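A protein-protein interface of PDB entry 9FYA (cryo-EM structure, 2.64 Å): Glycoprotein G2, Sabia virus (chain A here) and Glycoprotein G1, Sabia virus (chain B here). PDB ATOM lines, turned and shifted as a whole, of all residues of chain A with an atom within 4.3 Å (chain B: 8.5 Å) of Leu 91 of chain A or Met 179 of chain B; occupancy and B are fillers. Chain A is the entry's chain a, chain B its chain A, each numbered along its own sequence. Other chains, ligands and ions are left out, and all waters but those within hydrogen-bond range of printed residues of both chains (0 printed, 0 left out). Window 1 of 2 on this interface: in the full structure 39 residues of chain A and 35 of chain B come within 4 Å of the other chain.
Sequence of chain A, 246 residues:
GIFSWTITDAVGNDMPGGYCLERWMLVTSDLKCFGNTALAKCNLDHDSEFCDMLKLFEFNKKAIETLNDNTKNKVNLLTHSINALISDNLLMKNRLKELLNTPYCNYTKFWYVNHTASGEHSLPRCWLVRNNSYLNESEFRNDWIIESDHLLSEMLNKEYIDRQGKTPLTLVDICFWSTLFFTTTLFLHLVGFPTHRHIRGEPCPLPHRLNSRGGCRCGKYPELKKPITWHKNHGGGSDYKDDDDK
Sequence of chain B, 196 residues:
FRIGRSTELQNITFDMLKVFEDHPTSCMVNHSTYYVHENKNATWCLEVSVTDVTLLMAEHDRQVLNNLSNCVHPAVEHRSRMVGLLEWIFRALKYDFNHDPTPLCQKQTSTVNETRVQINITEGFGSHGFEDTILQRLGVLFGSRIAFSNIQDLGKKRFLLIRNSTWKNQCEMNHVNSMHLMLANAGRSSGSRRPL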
ATOM      1  N   MET A  53       1.266 -27.356  32.900  1.00  0.00           N
ATOM      2  CA  MET A  53       1.023 -25.965  32.527  1.00  0.00           C
ATOM      3  C   MET A  53       0.746 -25.125  33.767  1.00  0.00           C
ATOM      4  O   MET A  53       1.143 -23.958  33.841  1.00  0.00           O
ATOM      5  CB  MET A  53      -0.129 -25.870  31.522  1.00  0.00           C
ATOM      6  CG  MET A  53       0.125 -26.565  30.192  1.00  0.00           C
ATOM      7  SD  MET A  53       1.362 -25.789  29.126  1.00  0.00           S
ATOM      8  CE  MET A  53       2.878 -26.595  29.602  1.00  0.00           C
ATOM      9  N   ILE A  86       7.975 -29.278  33.658  1.00  0.00           N
ATOM     10  CA  ILE A  86       7.471 -29.924  32.452  1.00  0.00           C
ATOM     11  C   ILE A  86       8.040 -31.332  32.384  1.00  0.00           C
ATOM     12  O   ILE A  86       9.257 -31.521  32.489  1.00  0.00           O
ATOM     13  CB  ILE A  86       7.831 -29.117  31.192  1.00  0.00           C
ATOM     14  CG1 ILE A  86       7.180 -27.738  31.249  1.00  0.00           C
ATOM     15  CG2 ILE A  86       7.416 -29.847  29.934  1.00  0.00           C
ATOM     16  CD1 ILE A  86       5.694 -27.776  31.418  1.00  0.00           C
ATOM     17  N   SER A  87       7.167 -32.317  32.198  1.00  0.00           N
ATOM     18  CA  SER A  87       7.609 -33.691  32.014  1.00  0.00           C
ATOM     19  C   SER A  87       8.105 -33.854  30.584  1.00  0.00           C
ATOM     20  O   SER A  87       7.342 -33.671  29.631  1.00  0.00           O
ATOM     21  CB  SER A  87       6.469 -34.664  32.307  1.00  0.00           C
ATOM     22  OG  SER A  87       6.889 -36.009  32.162  1.00  0.00           O
ATOM     23  N   ASP A  88       9.388 -34.184  30.435  1.00  0.00           N
ATOM     24  CA  ASP A  88       9.954 -34.370  29.105  1.00  0.00           C
ATOM     25  C   ASP A  88       9.311 -35.552  28.390  1.00  0.00           C
ATOM     26  O   ASP A  88       9.077 -35.497  27.179  1.00  0.00           O
ATOM     27  CB  ASP A  88      11.468 -34.548  29.204  1.00  0.00           C
ATOM     28  CG  ASP A  88      12.200 -34.011  27.988  1.00  0.00           C
ATOM     29  OD1 ASP A  88      11.702 -34.186  26.856  1.00  0.00           O
ATOM     30  OD2 ASP A  88      13.281 -33.411  28.163  1.00  0.00           O
ATOM     31  N   ASN A  89       9.026 -36.631  29.122  1.00  0.00           N
ATOM     32  CA  ASN A  89       8.429 -37.812  28.508  1.00  0.00           C
ATOM     33  C   ASN A  89       7.039 -37.515  27.957  1.00  0.00           C
ATOM     34  O   ASN A  89       6.687 -37.980  26.870  1.00  0.00           O
ATOM     35  CB  ASN A  89       8.378 -38.967  29.508  1.00  0.00           C
ATOM     36  CG  ASN A  89       9.752 -39.364  30.012  1.00  0.00           C
ATOM     37  OD1 ASN A  89      10.528 -39.994  29.303  1.00  0.00           O
ATOM     38  ND2 ASN A  89      10.050 -39.009  31.248  1.00  0.00           N
ATOM     39  N   LEU A  90       6.226 -36.766  28.701  1.00  0.00           N
ATOM     40  CA  LEU A  90       4.884 -36.430  28.230  1.00  0.00           C
ATOM     41  C   LEU A  90       4.921 -35.538  26.993  1.00  0.00           C
ATOM     42  O   LEU A  90       4.169 -35.765  26.033  1.00  0.00           O
ATOM     43  CB  LEU A  90       4.096 -35.781  29.362  1.00  0.00           C
ATOM     44  CG  LEU A  90       2.584 -35.746  29.200  1.00  0.00           C
ATOM     45  CD1 LEU A  90       2.026 -37.135  29.289  1.00  0.00           C
ATOM     46  CD2 LEU A  90       2.015 -34.894  30.297  1.00  0.00           C
ATOM     47  N   LEU A  91       5.794 -34.528  26.993  1.00  0.00           N
ATOM     48  CA  LEU A  91       5.951 -33.680  25.817  1.00  0.00           C
ATOM     49  C   LEU A  91       6.415 -34.495  24.624  1.00  0.00           C
ATOM     50  O   LEU A  91       5.936 -34.304  23.501  1.00  0.00           O
ATOM     51  CB  LEU A  91       6.941 -32.553  26.116  1.00  0.00           C
ATOM     52  CG  LEU A  91       6.908 -31.269  25.284  1.00  0.00           C
ATOM     53  CD1 LEU A  91       5.807 -30.326  25.702  1.00  0.00           C
ATOM     54  CD2 LEU A  91       8.252 -30.591  25.380  1.00  0.00           C
ATOM     55  N   MET A  92       7.358 -35.406  24.853  1.00  0.00           N
ATOM     56  CA  MET A  92       7.861 -36.264  23.790  1.00  0.00           C
ATOM     57  C   MET A  92       6.765 -37.168  23.239  1.00  0.00           C
ATOM     58  O   MET A  92       6.665 -37.363  22.023  1.00  0.00           O
ATOM     59  CB  MET A  92       9.031 -37.086  24.319  1.00  0.00           C
ATOM     60  CG  MET A  92       9.833 -37.738  23.245  1.00  0.00           C
ATOM     61  SD  MET A  92      10.484 -36.512  22.113  1.00  0.00           S
ATOM     62  CE  MET A  92      10.202 -37.376  20.588  1.00  0.00           C
ATOM     63  N   LYS A  93       5.939 -37.736  24.119  1.00  0.00           N
ATOM     64  CA  LYS A  93       4.847 -38.583  23.657  1.00  0.00           C
ATOM     65  C   LYS A  93       3.873 -37.795  22.802  1.00  0.00           C
ATOM     66  O   LYS A  93       3.421 -38.279  21.761  1.00  0.00           O
ATOM     67  CB  LYS A  93       4.116 -39.217  24.837  1.00  0.00           C
ATOM     68  CG  LYS A  93       4.896 -40.298  25.540  1.00  0.00           C
ATOM     69  CD  LYS A  93       4.107 -40.901  26.687  1.00  0.00           C
ATOM     70  CE  LYS A  93       4.629 -40.434  28.030  1.00  0.00           C
ATOM     71  NZ  LYS A  93       4.132 -41.294  29.133  1.00  0.00           N
ATOM     72  N   ASN A  94       3.527 -36.582  23.230  1.00  0.00           N
ATOM     73  CA  ASN A  94       2.608 -35.776  22.435  1.00  0.00           C
ATOM     74  C   ASN A  94       3.216 -35.404  21.087  1.00  0.00           C
ATOM     75  O   ASN A  94       2.520 -35.401  20.067  1.00  0.00           O
ATOM     76  CB  ASN A  94       2.179 -34.543  23.222  1.00  0.00           C
ATOM     77  CG  ASN A  94       1.232 -34.886  24.340  1.00  0.00           C
ATOM     78  OD1 ASN A  94       0.183 -35.473  24.105  1.00  0.00           O
ATOM     79  ND2 ASN A  94       1.590 -34.525  25.561  1.00  0.00           N
ATOM     80  N   ARG A  95       4.513 -35.088  21.058  1.00  0.00           N
ATOM     81  CA  ARG A  95       5.156 -34.781  19.784  1.00  0.00           C
ATOM     82  C   ARG A  95       5.162 -35.988  18.852  1.00  0.00           C
ATOM     83  O   ARG A  95       4.907 -35.853  17.650  1.00  0.00           O
ATOM     84  CB  ARG A  95       6.582 -34.279  20.004  1.00  0.00           C
ATOM     85  CG  ARG A  95       7.294 -33.958  18.702  1.00  0.00           C
ATOM     86  CD  ARG A  95       6.680 -32.762  17.987  1.00  0.00           C
ATOM     87  NE  ARG A  95       7.183 -31.488  18.483  1.00  0.00           N
ATOM     88  CZ  ARG A  95       6.650 -30.308  18.206  1.00  0.00           C
ATOM     89  NH1 ARG A  95       5.572 -30.197  17.454  1.00  0.00           N
ATOM     90  NH2 ARG A  95       7.230 -29.209  18.670  1.00  0.00           N
ATOM     91  N   TYR A 107      -0.973 -28.524  24.391  1.00  0.00           N
ATOM     92  CA  TYR A 107      -0.809 -27.744  25.619  1.00  0.00           C
ATOM     93  C   TYR A 107      -1.536 -26.402  25.618  1.00  0.00           C
ATOM     94  O   TYR A 107      -1.139 -25.483  26.335  1.00  0.00           O
ATOM     95  CB  TYR A 107       0.677 -27.550  25.945  1.00  0.00           C
ATOM     96  CG  TYR A 107       1.383 -28.843  26.293  1.00  0.00           C
ATOM     97  CD1 TYR A 107       1.703 -29.774  25.316  1.00  0.00           C
ATOM     98  CD2 TYR A 107       1.706 -29.138  27.603  1.00  0.00           C
ATOM     99  CE1 TYR A 107       2.330 -30.954  25.636  1.00  0.00           C
ATOM    100  CE2 TYR A 107       2.337 -30.309  27.932  1.00  0.00           C
ATOM    101  CZ  TYR A 107       2.645 -31.215  26.948  1.00  0.00           C
ATOM    102  OH  TYR A 107       3.273 -32.381  27.293  1.00  0.00           O
ATOM    103  N   MET B  16       0.172 -18.181  26.560  1.00  0.00           N
ATOM    104  CA  MET B  16       1.552 -18.427  26.948  1.00  0.00           C
ATOM    105  C   MET B  16       2.484 -17.306  26.525  1.00  0.00           C
ATOM    106  O   MET B  16       3.702 -17.501  26.502  1.00  0.00           O
ATOM    107  CB  MET B  16       2.027 -19.759  26.372  1.00  0.00           C
ATOM    108  CG  MET B  16       1.184 -20.907  26.839  1.00  0.00           C
ATOM    109  SD  MET B  16       1.448 -21.181  28.592  1.00  0.00           S
ATOM    110  CE  MET B  16       0.445 -22.626  28.832  1.00  0.00           C
ATOM    111  N   VAL B  19       4.844 -16.068  29.539  1.00  0.00           N
ATOM    112  CA  VAL B  19       5.834 -17.051  29.969  1.00  0.00           C
ATOM    113  C   VAL B  19       6.985 -17.142  28.971  1.00  0.00           C
ATOM    114  O   VAL B  19       8.148 -17.269  29.362  1.00  0.00           O
ATOM    115  CB  VAL B  19       5.165 -18.417  30.200  1.00  0.00           C
ATOM    116  CG1 VAL B  19       6.197 -19.461  30.595  1.00  0.00           C
ATOM    117  CG2 VAL B  19       4.096 -18.302  31.266  1.00  0.00           C
ATOM    118  N   PHE B  20       6.685 -17.083  27.669  1.00  0.00           N
ATOM    119  CA  PHE B  20       7.699 -17.325  26.648  1.00  0.00           C
ATOM    120  C   PHE B  20       8.003 -16.103  25.787  1.00  0.00           C
ATOM    121  O   PHE B  20       8.544 -16.255  24.691  1.00  0.00           O
ATOM    122  CB  PHE B  20       7.264 -18.486  25.750  1.00  0.00           C
ATOM    123  CG  PHE B  20       7.106 -19.794  26.467  1.00  0.00           C
ATOM    124  CD1 PHE B  20       8.209 -20.575  26.757  1.00  0.00           C
ATOM    125  CD2 PHE B  20       5.857 -20.249  26.839  1.00  0.00           C
ATOM    126  CE1 PHE B  20       8.068 -21.780  27.406  1.00  0.00           C
ATOM    127  CE2 PHE B  20       5.713 -21.450  27.495  1.00  0.00           C
ATOM    128  CZ  PHE B  20       6.819 -22.217  27.778  1.00  0.00           C
ATOM    129  N   HIS B  23      12.141 -15.696  25.874  1.00  0.00           N
ATOM    130  CA  HIS B  23      12.916 -16.901  25.664  1.00  0.00           C
ATOM    131  C   HIS B  23      12.954 -17.266  24.187  1.00  0.00           C
ATOM    132  O   HIS B  23      12.076 -16.854  23.423  1.00  0.00           O
ATOM    133  CB  HIS B  23      12.343 -18.066  26.477  1.00  0.00           C
ATOM    134  CG  HIS B  23      12.337 -17.811  27.948  1.00  0.00           C
ATOM    135  ND1 HIS B  23      13.495 -17.720  28.687  1.00  0.00           N
ATOM    136  CD2 HIS B  23      11.321 -17.580  28.809  1.00  0.00           C
ATOM    137  CE1 HIS B  23      13.191 -17.473  29.947  1.00  0.00           C
ATOM    138  NE2 HIS B  23      11.878 -17.380  30.048  1.00  0.00           N
ATOM    139  N   PRO B  24      13.979 -17.991  23.741  1.00  0.00           N
ATOM    140  CA  PRO B  24      14.018 -18.415  22.340  1.00  0.00           C
ATOM    141  C   PRO B  24      12.820 -19.284  21.990  1.00  0.00           C
ATOM    142  O   PRO B  24      12.358 -20.098  22.790  1.00  0.00           O
ATOM    143  CB  PRO B  24      15.329 -19.199  22.247  1.00  0.00           C
ATOM    144  CG  PRO B  24      16.168 -18.634  23.311  1.00  0.00           C
ATOM    145  CD  PRO B  24      15.241 -18.300  24.433  1.00  0.00           C
ATOM    146  N   THR B  25      12.324 -19.101  20.774  1.00  0.00           N
ATOM    147  CA  THR B  25      11.167 -19.816  20.270  1.00  0.00           C
ATOM    148  C   THR B  25      11.460 -20.232  18.840  1.00  0.00           C
ATOM    149  O   THR B  25      12.436 -19.790  18.236  1.00  0.00           O
ATOM    150  CB  THR B  25       9.898 -18.954  20.354  1.00  0.00           C
ATOM    151  OG1 THR B  25       8.751 -19.735  20.005  1.00  0.00           O
ATOM    152  CG2 THR B  25      10.004 -17.759  19.423  1.00  0.00           C
ATOM    153  N   SER B  26      10.641 -21.134  18.307  1.00  0.00           N
ATOM    154  CA  SER B  26      10.792 -21.567  16.925  1.00  0.00           C
ATOM    155  C   SER B  26       9.420 -21.801  16.310  1.00  0.00           C
ATOM    156  O   SER B  26       8.411 -21.925  17.007  1.00  0.00           O
ATOM    157  CB  SER B  26      11.675 -22.818  16.804  1.00  0.00           C
ATOM    158  OG  SER B  26      11.220 -23.873  17.623  1.00  0.00           O
ATOM    159  N   TRP B  88      22.280 -22.663  20.803  1.00  0.00           N
ATOM    160  CA  TRP B  88      21.000 -23.220  21.232  1.00  0.00           C
ATOM    161  C   TRP B  88      20.429 -24.169  20.187  1.00  0.00           C
ATOM    162  O   TRP B  88      19.917 -25.239  20.524  1.00  0.00           O
ATOM    163  CB  TRP B  88      20.011 -22.101  21.541  1.00  0.00           C
ATOM    164  CG  TRP B  88      20.041 -21.651  22.963  1.00  0.00           C
ATOM    165  CD1 TRP B  88      21.101 -21.141  23.637  1.00  0.00           C
ATOM    166  CD2 TRP B  88      18.951 -21.679  23.888  1.00  0.00           C
ATOM    167  NE1 TRP B  88      20.746 -20.849  24.926  1.00  0.00           N
ATOM    168  CE2 TRP B  88      19.429 -21.170  25.106  1.00  0.00           C
ATOM    169  CE3 TRP B  88      17.620 -22.090  23.806  1.00  0.00           C
ATOM    170  CZ2 TRP B  88      18.623 -21.056  26.232  1.00  0.00           C
ATOM    171  CZ3 TRP B  88      16.827 -21.980  24.921  1.00  0.00           C
ATOM    172  CH2 TRP B  88      17.328 -21.468  26.119  1.00  0.00           C
ATOM    173  N   VAL B 140      10.946 -33.573  15.847  1.00  0.00           N
ATOM    174  CA  VAL B 140      10.746 -33.390  17.281  1.00  0.00           C
ATOM    175  C   VAL B 140      10.792 -31.910  17.649  1.00  0.00           C
ATOM    176  O   VAL B 140       9.977 -31.426  18.444  1.00  0.00           O
ATOM    177  CB  VAL B 140      11.792 -34.205  18.062  1.00  0.00           C
ATOM    178  CG1 VAL B 140      11.830 -33.793  19.522  1.00  0.00           C
ATOM    179  CG2 VAL B 140      11.531 -35.685  17.912  1.00  0.00           C
ATOM    180  N   LEU B 141      11.727 -31.166  17.062  1.00  0.00           N
ATOM    181  CA  LEU B 141      11.903 -29.755  17.376  1.00  0.00           C
ATOM    182  C   LEU B 141      10.751 -28.912  16.844  1.00  0.00           C
ATOM    183  O   LEU B 141      10.090 -28.196  17.602  1.00  0.00           O
ATOM    184  CB  LEU B 141      13.228 -29.262  16.801  1.00  0.00           C
ATOM    185  CG  LEU B 141      14.435 -29.186  17.734  1.00  0.00           C
ATOM    186  CD1 LEU B 141      15.618 -28.588  16.993  1.00  0.00           C
ATOM    187  CD2 LEU B 141      14.123 -28.424  19.006  1.00  0.00           C
ATOM    188  N   MET B 173       4.490 -17.429  17.352  1.00  0.00           N
ATOM    189  CA  MET B 173       5.213 -18.093  18.428  1.00  0.00           C
ATOM    190  C   MET B 173       4.473 -19.363  18.824  1.00  0.00           C
ATOM    191  O   MET B 173       3.244 -19.387  18.909  1.00  0.00           O
ATOM    192  CB  MET B 173       5.373 -17.144  19.626  1.00  0.00           C
ATOM    193  CG  MET B 173       6.271 -17.648  20.764  1.00  0.00           C
ATOM    194  SD  MET B 173       5.487 -18.623  22.059  1.00  0.00           S
ATOM    195  CE  MET B 173       4.436 -17.401  22.832  1.00  0.00           C
ATOM    196  N   ASN B 174       5.229 -20.428  19.058  1.00  0.00           N
ATOM    197  CA  ASN B 174       4.676 -21.730  19.408  1.00  0.00           C
ATOM    198  C   ASN B 174       5.356 -22.186  20.690  1.00  0.00           C
ATOM    199  O   ASN B 174       6.556 -22.470  20.685  1.00  0.00           O
ATOM    200  CB  ASN B 174       4.899 -22.726  18.268  1.00  0.00           C
ATOM    201  CG  ASN B 174       4.133 -24.007  18.449  1.00  0.00           C
ATOM    202  OD1 ASN B 174       4.391 -24.775  19.367  1.00  0.00           O
ATOM    203  ND2 ASN B 174       3.189 -24.255  17.557  1.00  0.00           N
ATOM    204  N   HIS B 175       4.607 -22.233  21.793  1.00  0.00           N
ATOM    205  CA  HIS B 175       5.249 -22.488  23.076  1.00  0.00           C
ATOM    206  C   HIS B 175       5.635 -23.949  23.263  1.00  0.00           C
ATOM    207  O   HIS B 175       6.472 -24.237  24.119  1.00  0.00           O
ATOM    208  CB  HIS B 175       4.345 -22.035  24.233  1.00  0.00           C
ATOM    209  CG  HIS B 175       3.059 -22.796  24.351  1.00  0.00           C
ATOM    210  ND1 HIS B 175       2.859 -23.772  25.304  1.00  0.00           N
ATOM    211  CD2 HIS B 175       1.905 -22.719  23.648  1.00  0.00           C
ATOM    212  CE1 HIS B 175       1.643 -24.266  25.178  1.00  0.00           C
ATOM    213  NE2 HIS B 175       1.043 -23.646  24.180  1.00  0.00           N
ATOM    214  N   VAL B 176       5.070 -24.868  22.476  1.00  0.00           N
ATOM    215  CA  VAL B 176       5.554 -26.247  22.465  1.00  0.00           C
ATOM    216  C   VAL B 176       6.952 -26.330  21.863  1.00  0.00           C
ATOM    217  O   VAL B 176       7.832 -27.023  22.389  1.00  0.00           O
ATOM    218  CB  VAL B 176       4.559 -27.156  21.723  1.00  0.00           C
ATOM    219  CG1 VAL B 176       4.917 -28.605  21.931  1.00  0.00           C
ATOM    220  CG2 VAL B 176       3.162 -26.905  22.236  1.00  0.00           C
ATOM    221  N   ASN B 177       7.178 -25.627  20.752  1.00  0.00           N
ATOM    222  CA  ASN B 177       8.517 -25.554  20.183  1.00  0.00           C
ATOM    223  C   ASN B 177       9.477 -24.873  21.147  1.00  0.00           C
ATOM    224  O   ASN B 177      10.641 -25.273  21.270  1.00  0.00           O
ATOM    225  CB  ASN B 177       8.480 -24.810  18.848  1.00  0.00           C
ATOM    226  CG  ASN B 177       7.736 -25.570  17.773  1.00  0.00           C
ATOM    227  OD1 ASN B 177       7.383 -26.729  17.948  1.00  0.00           O
ATOM    228  ND2 ASN B 177       7.540 -24.931  16.631  1.00  0.00           N
ATOM    229  N   SER B 178       8.996 -23.840  21.846  1.00  0.00           N
ATOM    230  CA  SER B 178       9.797 -23.177  22.866  1.00  0.00           C
ATOM    231  C   SER B 178      10.189 -24.147  23.967  1.00  0.00           C
ATOM    232  O   SER B 178      11.335 -24.145  24.422  1.00  0.00           O
ATOM    233  CB  SER B 178       9.018 -22.004  23.459  1.00  0.00           C
ATOM    234  OG  SER B 178       8.768 -21.010  22.493  1.00  0.00           O
ATOM    235  N   MET B 179       9.243 -24.976  24.417  1.00  0.00           N
ATOM    236  CA  MET B 179       9.536 -25.951  25.459  1.00  0.00           C
ATOM    237  C   MET B 179      10.552 -26.978  24.988  1.00  0.00           C
ATOM    238  O   MET B 179      11.460 -27.341  25.738  1.00  0.00           O
ATOM    239  CB  MET B 179       8.252 -26.634  25.925  1.00  0.00           C
ATOM    240  CG  MET B 179       7.390 -25.780  26.830  1.00  0.00           C
ATOM    241  SD  MET B 179       5.964 -26.657  27.489  1.00  0.00           S
ATOM    242  CE  MET B 179       4.772 -26.393  26.191  1.00  0.00           C
ATOM    243  N   HIS B 180      10.425 -27.456  23.749  1.00  0.00           N
ATOM    244  CA  HIS B 180      11.390 -28.424  23.228  1.00  0.00           C
ATOM    245  C   HIS B 180      12.789 -27.820  23.169  1.00  0.00           C
ATOM    246  O   HIS B 180      13.775 -28.439  23.597  1.00  0.00           O
ATOM    247  CB  HIS B 180      10.958 -28.910  21.842  1.00  0.00           C
ATOM    248  CG  HIS B 180       9.912 -29.983  21.872  1.00  0.00           C
ATOM    249  ND1 HIS B 180       8.587 -29.740  21.587  1.00  0.00           N
ATOM    250  CD2 HIS B 180      10.000 -31.305  22.146  1.00  0.00           C
ATOM    251  CE1 HIS B 180       7.903 -30.864  21.688  1.00  0.00           C
ATOM    252  NE2 HIS B 180       8.739 -31.830  22.024  1.00  0.00           N
ATOM    253  N   LEU B 181      12.886 -26.594  22.651  1.00  0.00           N
ATOM    254  CA  LEU B 181      14.165 -25.902  22.562  1.00  0.00           C
ATOM    255  C   LEU B 181      14.774 -25.656  23.939  1.00  0.00           C
ATOM    256  O   LEU B 181      15.968 -25.888  24.149  1.00  0.00           O
ATOM    257  CB  LEU B 181      13.955 -24.587  21.812  1.00  0.00           C
ATOM    258  CG  LEU B 181      15.088 -23.724  21.281  1.00  0.00           C
ATOM    259  CD1 LEU B 181      15.939 -24.471  20.302  1.00  0.00           C
ATOM    260  CD2 LEU B 181      14.463 -22.524  20.612  1.00  0.00           C
ATOM    261  N   MET B 182      13.968 -25.189  24.893  1.00  0.00           N
ATOM    262  CA  MET B 182      14.484 -24.906  26.228  1.00  0.00           C
ATOM    263  C   MET B 182      14.872 -26.180  26.965  1.00  0.00           C
ATOM    264  O   MET B 182      15.821 -26.176  27.752  1.00  0.00           O
ATOM    265  CB  MET B 182      13.467 -24.104  27.036  1.00  0.00           C
ATOM    266  CG  MET B 182      13.298 -22.679  26.558  1.00  0.00           C
ATOM    267  SD  MET B 182      12.205 -21.727  27.624  1.00  0.00           S
ATOM    268  CE  MET B 182      13.209 -21.660  29.105  1.00  0.00           C
ATOM    269  N   LEU B 183      14.123 -27.267  26.761  1.00  0.00           N
ATOM    270  CA  LEU B 183      14.490 -28.549  27.348  1.00  0.00           C
ATOM    271  C   LEU B 183      15.830 -29.026  26.814  1.00  0.00           C
ATOM    272  O   LEU B 183      16.644 -29.574  27.564  1.00  0.00           O
ATOM    273  CB  LEU B 183      13.403 -29.583  27.067  1.00  0.00           C
ATOM    274  CG  LEU B 183      12.188 -29.604  27.994  1.00  0.00           C
ATOM    275  CD1 LEU B 183      11.240 -30.713  27.597  1.00  0.00           C
ATOM    276  CD2 LEU B 183      12.619 -29.762  29.432  1.00  0.00           C
ATOM    277  N   ALA B 184      16.080 -28.828  25.519  1.00  0.00           N
ATOM    278  CA  ALA B 184      17.377 -29.199  24.969  1.00  0.00           C
ATOM    279  C   ALA B 184      18.510 -28.331  25.501  1.00  0.00           C
ATOM    280  O   ALA B 184      19.671 -28.741  25.434  1.00  0.00           O
ATOM    281  CB  ALA B 184      17.347 -29.125  23.450  1.00  0.00           C
ATOM    282  N   ASN B 185      18.204 -27.138  25.999  1.00  0.00           N
ATOM    283  CA  ASN B 185      19.188 -26.208  26.532  1.00  0.00           C
ATOM    284  C   ASN B 185      18.922 -25.900  27.998  1.00  0.00           C
ATOM    285  O   ASN B 185      19.002 -24.751  28.432  1.00  0.00           O
ATOM    286  CB  ASN B 185      19.212 -24.918  25.715  1.00  0.00           C
ATOM    287  CG  ASN B 185      19.603 -25.149  24.276  1.00  0.00           C
ATOM    288  OD1 ASN B 185      20.773 -25.065  23.924  1.00  0.00           O
ATOM    289  ND2 ASN B 185      18.624 -25.445  23.436  1.00  0.00           N
ATOM    290  N   ALA B 186      18.583 -26.919  28.778  1.00  0.00           N
ATOM    291  CA  ALA B 186      18.316 -26.704  30.191  1.00  0.00           C
ATOM    292  C   ALA B 186      19.593 -26.288  30.908  1.00  0.00           C
ATOM    293  O   ALA B 186      20.665 -26.856  30.687  1.00  0.00           O
ATOM    294  CB  ALA B 186      17.735 -27.966  30.820  1.00  0.00           C
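The guanidinium group of Arg 95 of chain A is in hydrogen-bond range of the backbone carbonyl oxygen of Val 140 of chain B (2.8 Å).
NH2 of Arg 95 of chain A lies within hydrogen-bond range of O of Leu 141 of chain B, 3.2 Å away.
NH2 of Arg 95 of chain A sits at hydrogen-bond distance from OD1 of Asn 177 of chain B (2.6 Å).
A ring nitrogen (ND1) of His 180 of chain B sits at hydrogen-bond distance from the guanidinium group of Arg 95 of chain A, 3.3 Å away.
ND2 of Asn 94 of chain A is in hydrogen-bond range of OH of Tyr 107 of chain A (3.2 Å).
The backbone carbonyl oxygen of Ser 26 of chain B is in hydrogen-bond range of the side-chain amide nitrogen of Asn 177 of chain B, 3.2 Å away.
OD1 of Asn 177 of chain B sits close to O of Leu 141 of chain B (3.1 Å).
The side-chain sulfur (SD) of Met 173 of chain B sits at hydrogen-bond distance from the backbone NH (N) of His 175 of chain B (3.7 Å).
OD1 of Asn 174 of chain B is in hydrogen-bond range of N of Asn 177 of chain B, 3.2 Å away.
A ring nitrogen (ND1) of His 180 of chain B lies within hydrogen-bond range of the backbone carbonyl oxygen (O) of Val 176 of chain B.
Met 53 of chain A touches Met 16 of chain B (SD to CE, 3.3 Å).
CE of Met 53 of chain A touches SD of Met 179 of chain B (3.7 Å).
Asp 88 of chain A touches Leu 183 of chain B.
CB of Met 179 of chain B touches CD2 of Leu 91 of chain A (3.99 Å).
Leu 91 of chain A touches His 180 of chain B.
Leu 91 of chain A touches Leu 183 of chain B.
Met 92 of chain A touches Val 140 of chain B (CE to CG2, 3.4 Å).
CE1 of His 175 of chain B touches O of Tyr 107 of chain A, 3.2 Å away.
Of the printed residues of chain B, Leu 91 of chain A touches Met 179, His 180 and Leu 183.
Printed residues of chain A within 4 Å of Met 179 of chain B: Met 53 (3.7 Å) and Leu 91 (3.99 Å).
Printed residues of chain B within 4 Å of Tyr 107 of chain A: His 175.
Of the printed residues of chain A, Val 140 of chain B touches Met 92 and Arg 95.
Of the printed residues of chain A, Met 16 of chain B touches Met 53 (3.3 Å).
Of the printed residues of chain B, Arg 95 of chain A touches Val 140, Leu 141, Asn 177 and His 180.
Printed residues of chain A within 4 Å of His 180 of chain B: Leu 91 (3.6 Å) and Arg 95 (3.3 Å).
Printed residues of chain A that touch a printed residue of chain B: Met 53, Asp 88, Leu 91, Met 92, Arg 95 and Tyr 107.
Hydrophobic or aromatic side chains of chain A that line the printed part of chain B: Met 53, Leu 91, Met 92 and Tyr 107.
Among the printed residues, no Asp or Glu carboxylate lies within 4 Å of a Lys or Arg side-chain nitrogen of the other chain.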
